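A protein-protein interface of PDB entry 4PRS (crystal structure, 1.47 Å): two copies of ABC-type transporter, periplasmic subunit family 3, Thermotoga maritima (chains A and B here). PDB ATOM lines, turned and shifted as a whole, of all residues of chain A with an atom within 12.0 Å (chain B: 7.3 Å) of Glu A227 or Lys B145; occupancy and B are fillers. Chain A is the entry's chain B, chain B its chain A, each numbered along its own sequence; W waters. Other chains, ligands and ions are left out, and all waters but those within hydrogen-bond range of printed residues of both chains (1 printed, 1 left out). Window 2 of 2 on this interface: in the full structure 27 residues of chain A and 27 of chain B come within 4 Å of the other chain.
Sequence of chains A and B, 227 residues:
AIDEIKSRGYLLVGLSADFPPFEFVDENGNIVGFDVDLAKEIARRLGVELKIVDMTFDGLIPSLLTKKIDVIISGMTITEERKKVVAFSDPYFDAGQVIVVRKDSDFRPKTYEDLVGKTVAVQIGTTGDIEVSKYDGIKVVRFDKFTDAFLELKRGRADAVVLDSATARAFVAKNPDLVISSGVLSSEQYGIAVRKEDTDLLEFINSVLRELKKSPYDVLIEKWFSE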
ATOM      1  N   ASP A 218     -24.304  15.890  32.200  1.00  0.00           N
ATOM      2  CA  ASP A 218     -23.039  16.526  32.277  1.00  0.00           C
ATOM      3  C   ASP A 218     -21.921  15.525  32.548  1.00  0.00           C
ATOM      4  O   ASP A 218     -20.818  15.643  31.991  1.00  0.00           O
ATOM      5  CB  ASP A 218     -23.037  17.567  33.436  1.00  0.00           C
ATOM      6  CG  ASP A 218     -23.981  18.715  33.167  1.00  0.00           C
ATOM      7  OD1 ASP A 218     -24.249  19.133  31.983  1.00  0.00           O
ATOM      8  OD2 ASP A 218     -24.426  19.276  34.195  1.00  0.00           O
ATOM      9  N   VAL A 219     -22.192  14.552  33.388  1.00  0.00           N
ATOM     10  CA  VAL A 219     -21.207  13.499  33.721  1.00  0.00           C
ATOM     11  C   VAL A 219     -20.948  12.614  32.487  1.00  0.00           C
ATOM     12  O   VAL A 219     -19.799  12.250  32.208  1.00  0.00           O
ATOM     13  CB  VAL A 219     -21.703  12.682  34.905  1.00  0.00           C
ATOM     14  CG1 VAL A 219     -20.852  11.476  35.184  1.00  0.00           C
ATOM     15  CG2 VAL A 219     -21.808  13.670  36.157  1.00  0.00           C
ATOM     16  N   LEU A 220     -21.996  12.352  31.693  1.00  0.00           N
ATOM     17  CA  LEU A 220     -21.836  11.591  30.451  1.00  0.00           C
ATOM     18  C   LEU A 220     -20.987  12.361  29.445  1.00  0.00           C
ATOM     19  O   LEU A 220     -20.140  11.766  28.756  1.00  0.00           O
ATOM     20  CB  LEU A 220     -23.203  11.307  29.858  1.00  0.00           C
ATOM     21  CG  LEU A 220     -23.903  10.069  30.374  1.00  0.00           C
ATOM     22  CD1 LEU A 220     -25.268   9.962  29.729  1.00  0.00           C
ATOM     23  CD2 LEU A 220     -23.072   8.828  30.014  1.00  0.00           C
ATOM     24  N   ILE A 221     -21.194  13.683  29.330  1.00  0.00           N
ATOM     25  CA  ILE A 221     -20.349  14.526  28.481  1.00  0.00           C
ATOM     26  C   ILE A 221     -18.890  14.402  28.948  1.00  0.00           C
ATOM     27  O   ILE A 221     -17.958  14.230  28.140  1.00  0.00           O
ATOM     28  CB  ILE A 221     -20.814  15.993  28.461  1.00  0.00           C
ATOM     29  CG1 ILE A 221     -22.161  16.121  27.720  1.00  0.00           C
ATOM     30  CG2 ILE A 221     -19.737  16.850  27.869  1.00  0.00           C
ATOM     31  CD1 ILE A 221     -22.141  15.973  26.202  1.00  0.00           C
ATOM     32  N   GLU A 222     -18.692  14.513  30.235  1.00  0.00           N
ATOM     33  CA  GLU A 222     -17.340  14.414  30.771  1.00  0.00           C
ATOM     34  C   GLU A 222     -16.742  13.063  30.452  1.00  0.00           C
ATOM     35  O   GLU A 222     -15.542  12.967  30.091  1.00  0.00           O
ATOM     36  CB  GLU A 222     -17.373  14.614  32.274  1.00  0.00           C
ATOM     37  CG  GLU A 222     -17.509  16.049  32.676  1.00  0.00           C
ATOM     38  CD  GLU A 222     -17.684  16.244  34.200  1.00  0.00           C
ATOM     39  OE1 GLU A 222     -17.921  15.261  34.976  1.00  0.00           O
ATOM     40  OE2 GLU A 222     -17.596  17.409  34.634  1.00  0.00           O
ATOM     41  N   LYS A 223     -17.560  11.997  30.543  1.00  0.00           N
ATOM     42  CA  LYS A 223     -17.041  10.643  30.276  1.00  0.00           C
ATOM     43  C   LYS A 223     -16.474  10.520  28.833  1.00  0.00           C
ATOM     44  O   LYS A 223     -15.433   9.933  28.629  1.00  0.00           O
ATOM     45  CB  LYS A 223     -18.136   9.597  30.577  1.00  0.00           C
ATOM     46  CG  LYS A 223     -17.688   8.164  30.234  1.00  0.00           C
ATOM     47  CD  LYS A 223     -18.812   7.178  30.433  1.00  0.00           C
ATOM     48  CE  LYS A 223     -18.409   5.774  30.115  1.00  0.00           C
ATOM     49  NZ  LYS A 223     -19.602   4.784  30.203  1.00  0.00           N
ATOM     50  N   TRP A 224     -17.192  11.103  27.873  1.00  0.00           N
ATOM     51  CA  TRP A 224     -16.899  10.827  26.458  1.00  0.00           C
ATOM     52  C   TRP A 224     -16.107  11.903  25.742  1.00  0.00           C
ATOM     53  O   TRP A 224     -15.560  11.644  24.650  1.00  0.00           O
ATOM     54  CB  TRP A 224     -18.183  10.509  25.647  1.00  0.00           C
ATOM     55  CG  TRP A 224     -18.744   9.204  26.138  1.00  0.00           C
ATOM     56  CD1 TRP A 224     -19.824   9.021  26.921  1.00  0.00           C
ATOM     57  CD2 TRP A 224     -18.177   7.898  25.896  1.00  0.00           C
ATOM     58  NE1 TRP A 224     -19.995   7.675  27.163  1.00  0.00           N
ATOM     59  CE2 TRP A 224     -19.015   6.964  26.501  1.00  0.00           C
ATOM     60  CE3 TRP A 224     -17.092   7.453  25.133  1.00  0.00           C
ATOM     61  CZ2 TRP A 224     -18.728   5.554  26.524  1.00  0.00           C
ATOM     62  CZ3 TRP A 224     -16.759   6.098  25.132  1.00  0.00           C
ATOM     63  CH2 TRP A 224     -17.584   5.140  25.816  1.00  0.00           C
ATOM     64  N   PHE A 225     -16.000  13.085  26.356  1.00  0.00           N
ATOM     65  CA  PHE A 225     -15.363  14.228  25.676  1.00  0.00           C
ATOM     66  C   PHE A 225     -14.188  14.766  26.449  1.00  0.00           C
ATOM     67  O   PHE A 225     -13.739  15.807  26.164  1.00  0.00           O
ATOM     68  CB  PHE A 225     -16.426  15.320  25.416  1.00  0.00           C
ATOM     69  CG  PHE A 225     -17.451  14.893  24.404  1.00  0.00           C
ATOM     70  CD1 PHE A 225     -17.211  15.019  23.018  1.00  0.00           C
ATOM     71  CD2 PHE A 225     -18.602  14.216  24.850  1.00  0.00           C
ATOM     72  CE1 PHE A 225     -18.136  14.540  22.111  1.00  0.00           C
ATOM     73  CE2 PHE A 225     -19.521  13.702  23.944  1.00  0.00           C
ATOM     74  CZ  PHE A 225     -19.232  13.889  22.532  1.00  0.00           C
ATOM     75  N   SER A 226     -13.694  14.030  27.409  1.00  0.00           N
ATOM     76  CA  SER A 226     -12.475  14.380  28.143  1.00  0.00           C
ATOM     77  C   SER A 226     -11.220  13.728  27.514  1.00  0.00           C
ATOM     78  O   SER A 226     -11.322  12.917  26.583  1.00  0.00           O
ATOM     79  CB  SER A 226     -12.644  14.071  29.654  1.00  0.00           C
ATOM     80  OG  SER A 226     -12.887  12.683  29.944  1.00  0.00           O
ATOM     81  N   GLU A 227     -10.095  13.992  28.174  1.00  0.00           N
ATOM     82  CA  GLU A 227      -8.781  13.610  27.688  1.00  0.00           C
ATOM     83  C   GLU A 227      -7.987  12.916  28.786  1.00  0.00           C
ATOM     84  O   GLU A 227      -7.973  13.367  29.934  1.00  0.00           O
ATOM     85  CB  GLU A 227      -8.018  14.844  27.203  1.00  0.00           C
ATOM     86  CG  GLU A 227      -7.007  14.550  26.103  1.00  0.00           C
ATOM     87  CD  GLU A 227      -6.684  15.769  25.247  1.00  0.00           C
ATOM     88  OE1 GLU A 227      -6.298  16.811  25.810  1.00  0.00           O
ATOM     89  OE2 GLU A 227      -6.816  15.677  24.006  1.00  0.00           O
ATOM     90  N   VAL B 122      -5.055  23.603  16.795  1.00  0.00           N
ATOM     91  CA  VAL B 122      -6.088  22.571  16.646  1.00  0.00           C
ATOM     92  C   VAL B 122      -5.521  21.262  17.067  1.00  0.00           C
ATOM     93  O   VAL B 122      -4.286  21.103  17.223  1.00  0.00           O
ATOM     94  CB  VAL B 122      -6.528  22.410  15.140  1.00  0.00           C
ATOM     95  CG1 VAL B 122      -7.133  23.753  14.582  1.00  0.00           C
ATOM     96  CG2 VAL B 122      -5.327  21.978  14.234  1.00  0.00           C
ATOM     97  N   GLN B 123      -6.441  20.344  17.386  1.00  0.00           N
ATOM     98  CA  GLN B 123      -6.055  18.971  17.705  1.00  0.00           C
ATOM     99  C   GLN B 123      -5.981  18.169  16.416  1.00  0.00           C
ATOM    100  O   GLN B 123      -6.889  18.230  15.539  1.00  0.00           O
ATOM    101  CB  GLN B 123      -7.094  18.370  18.675  1.00  0.00           C
ATOM    102  CG  GLN B 123      -6.723  16.881  18.920  1.00  0.00           C
ATOM    103  CD  GLN B 123      -7.619  16.229  19.965  1.00  0.00           C
ATOM    104  OE1 GLN B 123      -8.755  16.634  20.150  1.00  0.00           O
ATOM    105  NE2 GLN B 123      -7.099  15.172  20.633  1.00  0.00           N
ATOM    106  N   ILE B 124      -4.856  17.502  16.252  1.00  0.00           N
ATOM    107  CA  ILE B 124      -4.640  16.716  15.019  1.00  0.00           C
ATOM    108  C   ILE B 124      -5.787  15.833  14.619  1.00  0.00           C
ATOM    109  O   ILE B 124      -6.328  15.041  15.430  1.00  0.00           O
ATOM    110  CB  ILE B 124      -3.366  15.781  15.171  1.00  0.00           C
ATOM    111  CG1 ILE B 124      -2.121  16.609  15.261  1.00  0.00           C
ATOM    112  CG2 ILE B 124      -3.211  14.829  13.940  1.00  0.00           C
ATOM    113  CD1 ILE B 124      -0.939  15.782  15.855  1.00  0.00           C
ATOM    114  N   ARG B 142      -0.540  22.231  15.147  1.00  0.00           N
ATOM    115  CA  ARG B 142      -1.311  21.000  15.439  1.00  0.00           C
ATOM    116  C   ARG B 142      -0.820  20.234  16.657  1.00  0.00           C
ATOM    117  O   ARG B 142       0.383  20.040  16.816  1.00  0.00           O
ATOM    118  CB  ARG B 142      -1.315  20.109  14.204  1.00  0.00           C
ATOM    119  CG  ARG B 142      -1.988  20.803  13.039  1.00  0.00           C
ATOM    120  CD  ARG B 142      -1.864  19.931  11.809  1.00  0.00           C
ATOM    121  NE  ARG B 142      -2.608  20.566  10.685  1.00  0.00           N
ATOM    122  CZ  ARG B 142      -2.067  21.547   9.970  1.00  0.00           C
ATOM    123  NH1 ARG B 142      -0.828  21.920  10.227  1.00  0.00           N
ATOM    124  NH2 ARG B 142      -2.755  22.127   9.021  1.00  0.00           N
ATOM    125  N   PHE B 143      -1.761  19.801  17.485  1.00  0.00           N
ATOM    126  CA  PHE B 143      -1.373  19.104  18.742  1.00  0.00           C
ATOM    127  C   PHE B 143      -2.045  17.765  18.841  1.00  0.00           C
ATOM    128  O   PHE B 143      -3.221  17.615  18.522  1.00  0.00           O
ATOM    129  CB  PHE B 143      -1.868  19.973  19.892  1.00  0.00           C
ATOM    130  CG  PHE B 143      -1.103  21.283  19.998  1.00  0.00           C
ATOM    131  CD1 PHE B 143      -1.417  22.387  19.200  1.00  0.00           C
ATOM    132  CD2 PHE B 143       0.014  21.346  20.820  1.00  0.00           C
ATOM    133  CE1 PHE B 143      -0.586  23.590  19.270  1.00  0.00           C
ATOM    134  CE2 PHE B 143       0.768  22.481  20.892  1.00  0.00           C
ATOM    135  CZ  PHE B 143       0.481  23.631  20.073  1.00  0.00           C
ATOM    136  N   ASP B 144      -1.305  16.820  19.376  1.00  0.00           N
ATOM    137  CA  ASP B 144      -1.859  15.513  19.668  1.00  0.00           C
ATOM    138  C   ASP B 144      -3.074  15.588  20.579  1.00  0.00           C
ATOM    139  O   ASP B 144      -4.147  14.954  20.279  1.00  0.00           O
ATOM    140  CB  ASP B 144      -0.723  14.683  20.278  1.00  0.00           C
ATOM    141  CG  ASP B 144      -1.143  13.252  20.639  1.00  0.00           C
ATOM    142  OD1 ASP B 144      -1.859  12.652  19.829  1.00  0.00           O
ATOM    143  OD2 ASP B 144      -0.693  12.747  21.693  1.00  0.00           O
ATOM    144  N   LYS B 145      -2.960  16.363  21.645  1.00  0.00           N
ATOM    145  CA  LYS B 145      -4.017  16.504  22.660  1.00  0.00           C
ATOM    146  C   LYS B 145      -4.637  17.906  22.587  1.00  0.00           C
ATOM    147  O   LYS B 145      -3.936  18.919  22.492  1.00  0.00           O
ATOM    148  CB  LYS B 145      -3.458  16.259  24.073  1.00  0.00           C
ATOM    149  CG  LYS B 145      -2.783  14.852  24.260  1.00  0.00           C
ATOM    150  CD  LYS B 145      -3.781  13.670  24.104  1.00  0.00           C
ATOM    151  CE  LYS B 145      -3.098  12.235  24.207  1.00  0.00           C
ATOM    152  NZ  LYS B 145      -4.138  11.159  24.087  1.00  0.00           N
ATOM    153  N   PHE B 146      -5.965  17.952  22.651  1.00  0.00           N
ATOM    154  CA  PHE B 146      -6.621  19.279  22.652  1.00  0.00           C
ATOM    155  C   PHE B 146      -6.214  20.109  23.850  1.00  0.00           C
ATOM    156  O   PHE B 146      -6.169  21.336  23.688  1.00  0.00           O
ATOM    157  CB  PHE B 146      -8.152  19.229  22.449  1.00  0.00           C
ATOM    158  CG  PHE B 146      -8.911  18.648  23.629  1.00  0.00           C
ATOM    159  CD1 PHE B 146      -9.019  19.396  24.810  1.00  0.00           C
ATOM    160  CD2 PHE B 146      -9.397  17.316  23.576  1.00  0.00           C
ATOM    161  CE1 PHE B 146      -9.734  18.910  25.935  1.00  0.00           C
ATOM    162  CE2 PHE B 146     -10.101  16.764  24.751  1.00  0.00           C
ATOM    163  CZ  PHE B 146     -10.233  17.567  25.911  1.00  0.00           C
ATOM    164  N   THR B 147      -5.905  19.506  25.018  1.00  0.00           N
ATOM    165  CA  THR B 147      -5.487  20.321  26.152  1.00  0.00           C
ATOM    166  C   THR B 147      -4.233  21.140  25.767  1.00  0.00           C
ATOM    167  O   THR B 147      -4.110  22.336  26.148  1.00  0.00           O
ATOM    168  CB  THR B 147      -5.229  19.428  27.389  1.00  0.00           C
ATOM    169  OG1 THR B 147      -6.472  18.794  27.742  1.00  0.00           O
ATOM    170  CG2 THR B 147      -4.756  20.282  28.624  1.00  0.00           C
ATOM    171  N   ASP B 148      -3.301  20.497  25.054  1.00  0.00           N
ATOM    172  CA  ASP B 148      -2.053  21.250  24.693  1.00  0.00           C
ATOM    173  C   ASP B 148      -2.313  22.362  23.662  1.00  0.00           C
ATOM    174  O   ASP B 148      -1.645  23.408  23.716  1.00  0.00           O
ATOM    175  CB  ASP B 148      -0.955  20.291  24.205  1.00  0.00           C
ATOM    176  CG  ASP B 148      -0.508  19.330  25.311  1.00  0.00           C
ATOM    177  OD1 ASP B 148      -0.279  19.850  26.403  1.00  0.00           O
ATOM    178  OD2 ASP B 148      -0.380  18.127  25.044  1.00  0.00           O
ATOM    179  N   ALA B 149      -3.329  22.203  22.803  1.00  0.00           N
ATOM    180  CA  ALA B 149      -3.740  23.355  21.920  1.00  0.00           C
ATOM    181  C   ALA B 149      -4.265  24.501  22.804  1.00  0.00           C
ATOM    182  O   ALA B 149      -3.920  25.682  22.560  1.00  0.00           O
ATOM    183  CB  ALA B 149      -4.814  22.852  20.945  1.00  0.00           C
ATOM    184  N   PHE B 150      -5.149  24.197  23.798  1.00  0.00           N
ATOM    185  CA  PHE B 150      -5.490  25.276  24.726  1.00  0.00           C
ATOM    186  C   PHE B 150      -4.321  25.907  25.502  1.00  0.00           C
ATOM    187  O   PHE B 150      -4.324  27.147  25.789  1.00  0.00           O
ATOM    188  CB  PHE B 150      -6.501  24.709  25.726  1.00  0.00           C
ATOM    189  CG  PHE B 150      -7.853  24.512  25.138  1.00  0.00           C
ATOM    190  CD1 PHE B 150      -8.518  25.589  24.541  1.00  0.00           C
ATOM    191  CD2 PHE B 150      -8.459  23.270  25.201  1.00  0.00           C
ATOM    192  CE1 PHE B 150      -9.837  25.410  23.997  1.00  0.00           C
ATOM    193  CE2 PHE B 150      -9.752  23.060  24.680  1.00  0.00           C
ATOM    194  CZ  PHE B 150     -10.457  24.108  24.114  1.00  0.00           C
ATOM    195  N   LEU B 151      -3.362  25.083  25.895  1.00  0.00           N
ATOM    196  CA  LEU B 151      -2.176  25.624  26.637  1.00  0.00           C
ATOM    197  C   LEU B 151      -1.354  26.522  25.735  1.00  0.00           C
ATOM    198  O   LEU B 151      -0.908  27.592  26.170  1.00  0.00           O
ATOM    199  CB  LEU B 151      -1.338  24.519  27.206  1.00  0.00           C
ATOM    200  CG  LEU B 151      -2.078  23.640  28.234  1.00  0.00           C
ATOM    201  CD1 LEU B 151      -1.028  22.745  28.953  1.00  0.00           C
ATOM    202  CD2 LEU B 151      -2.771  24.459  29.338  1.00  0.00           C
ATOM    203  N   THR B 167     -16.649  19.745  23.790  1.00  0.00           N
ATOM    204  CA  THR B 167     -15.394  19.603  24.469  1.00  0.00           C
ATOM    205  C   THR B 167     -14.920  21.001  24.845  1.00  0.00           C
ATOM    206  O   THR B 167     -14.422  21.208  25.943  1.00  0.00           O
ATOM    207  CB  THR B 167     -14.376  18.908  23.513  1.00  0.00           C
ATOM    208  OG1 THR B 167     -14.930  17.667  23.015  1.00  0.00           O
ATOM    209  CG2 THR B 167     -13.084  18.674  24.202  1.00  0.00           C
ATOM    210  N   PHE B 171     -14.157  22.519  28.561  1.00  0.00           N
ATOM    211  CA  PHE B 171     -12.823  23.013  28.999  1.00  0.00           C
ATOM    212  C   PHE B 171     -12.826  24.454  29.509  1.00  0.00           C
ATOM    213  O   PHE B 171     -12.126  24.791  30.486  1.00  0.00           O
ATOM    214  CB  PHE B 171     -11.838  22.955  27.795  1.00  0.00           C
ATOM    215  CG  PHE B 171     -10.370  23.243  28.186  1.00  0.00           C
ATOM    216  CD1 PHE B 171      -9.564  22.196  28.651  1.00  0.00           C
ATOM    217  CD2 PHE B 171      -9.820  24.539  28.099  1.00  0.00           C
ATOM    218  CE1 PHE B 171      -8.217  22.412  29.045  1.00  0.00           C
ATOM    219  CE2 PHE B 171      -8.478  24.756  28.485  1.00  0.00           C
ATOM    220  CZ  PHE B 171      -7.647  23.688  28.937  1.00  0.00           C
HETATM  221  O   HOH W   1      -8.260  13.655  22.910  1.00  0.00           O
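The side-chain carboxylate of Glu A227 is in hydrogen-bond range of the side-chain amide nitrogen of Gln B123, at 3.4 Å.
The backbone NH (N) of Phe B146 sits at hydrogen-bond distance from the side-chain carboxylate (OE2) of Glu A227 (2.8 Å).
The side-chain carboxylate (OE1) of Glu A227 lies within hydrogen-bond range of the side-chain hydroxyl (OG1) of Thr B147 (2.8 Å).
The side-chain amide nitrogen (NE2) of Gln B123 lies within hydrogen-bond range of the backbone carbonyl oxygen (O) of Asp B144 (3.0 Å).
Among the printed residues, merely in contact across the chains: Phe A225 with Phe B146, Phe A225 with Thr B167 and Glu A227 with Lys B145.
Glu A227 touches just these residues of chain B: Gln B123, Lys B145, Phe B146 and Thr B147.
Lys B145 touches one residue of chain A.
Of chain A, only Glu A227 comes within 4 Å of Gln B123.
Phe B143 touches none of the printed residues of chain A.
No residue of chain A comes within 4 Å of Asp B144.
No residue of chain A comes within 4 Å of Ala B149.
Of the printed residues of chain A, Thr B167 touches Phe A225.
Of the printed residues of chain B, Phe A225 touches Phe B146 and Thr B167.
The nearest printed residue of chain A that does not touch Lys B145 is Ser A226 (7.8 Å).
Of the 15 printed residues of chain B, 5 touch a printed residue of chain A.
Hydrophobic or aromatic side chains of chain B that line the printed part of chain A: Phe B146.
Along chain B the printed residues that touch a printed residue of chain A span positions 123 to 167.
Hydrophobic or aromatic side chains of chain A within 4 Å of the printed part of chain B: Phe A225.
Among the printed residues, 6 pairs touch across the chains.
Among the printed residues, no Asp or Glu carboxylate lies within 4 Å of a Lys or Arg side-chain nitrogen of the other chain.
No position is printed for both chains.
Of the 6 pairs that touch across the chains among the printed residues, none has its exchanged pair printed and touching as well.
Water W1 lies within hydrogen-bond range of the side-chain carboxylate (OE2) of Glu A227 and the side-chain amide nitrogen (NE2) of Gln B123.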
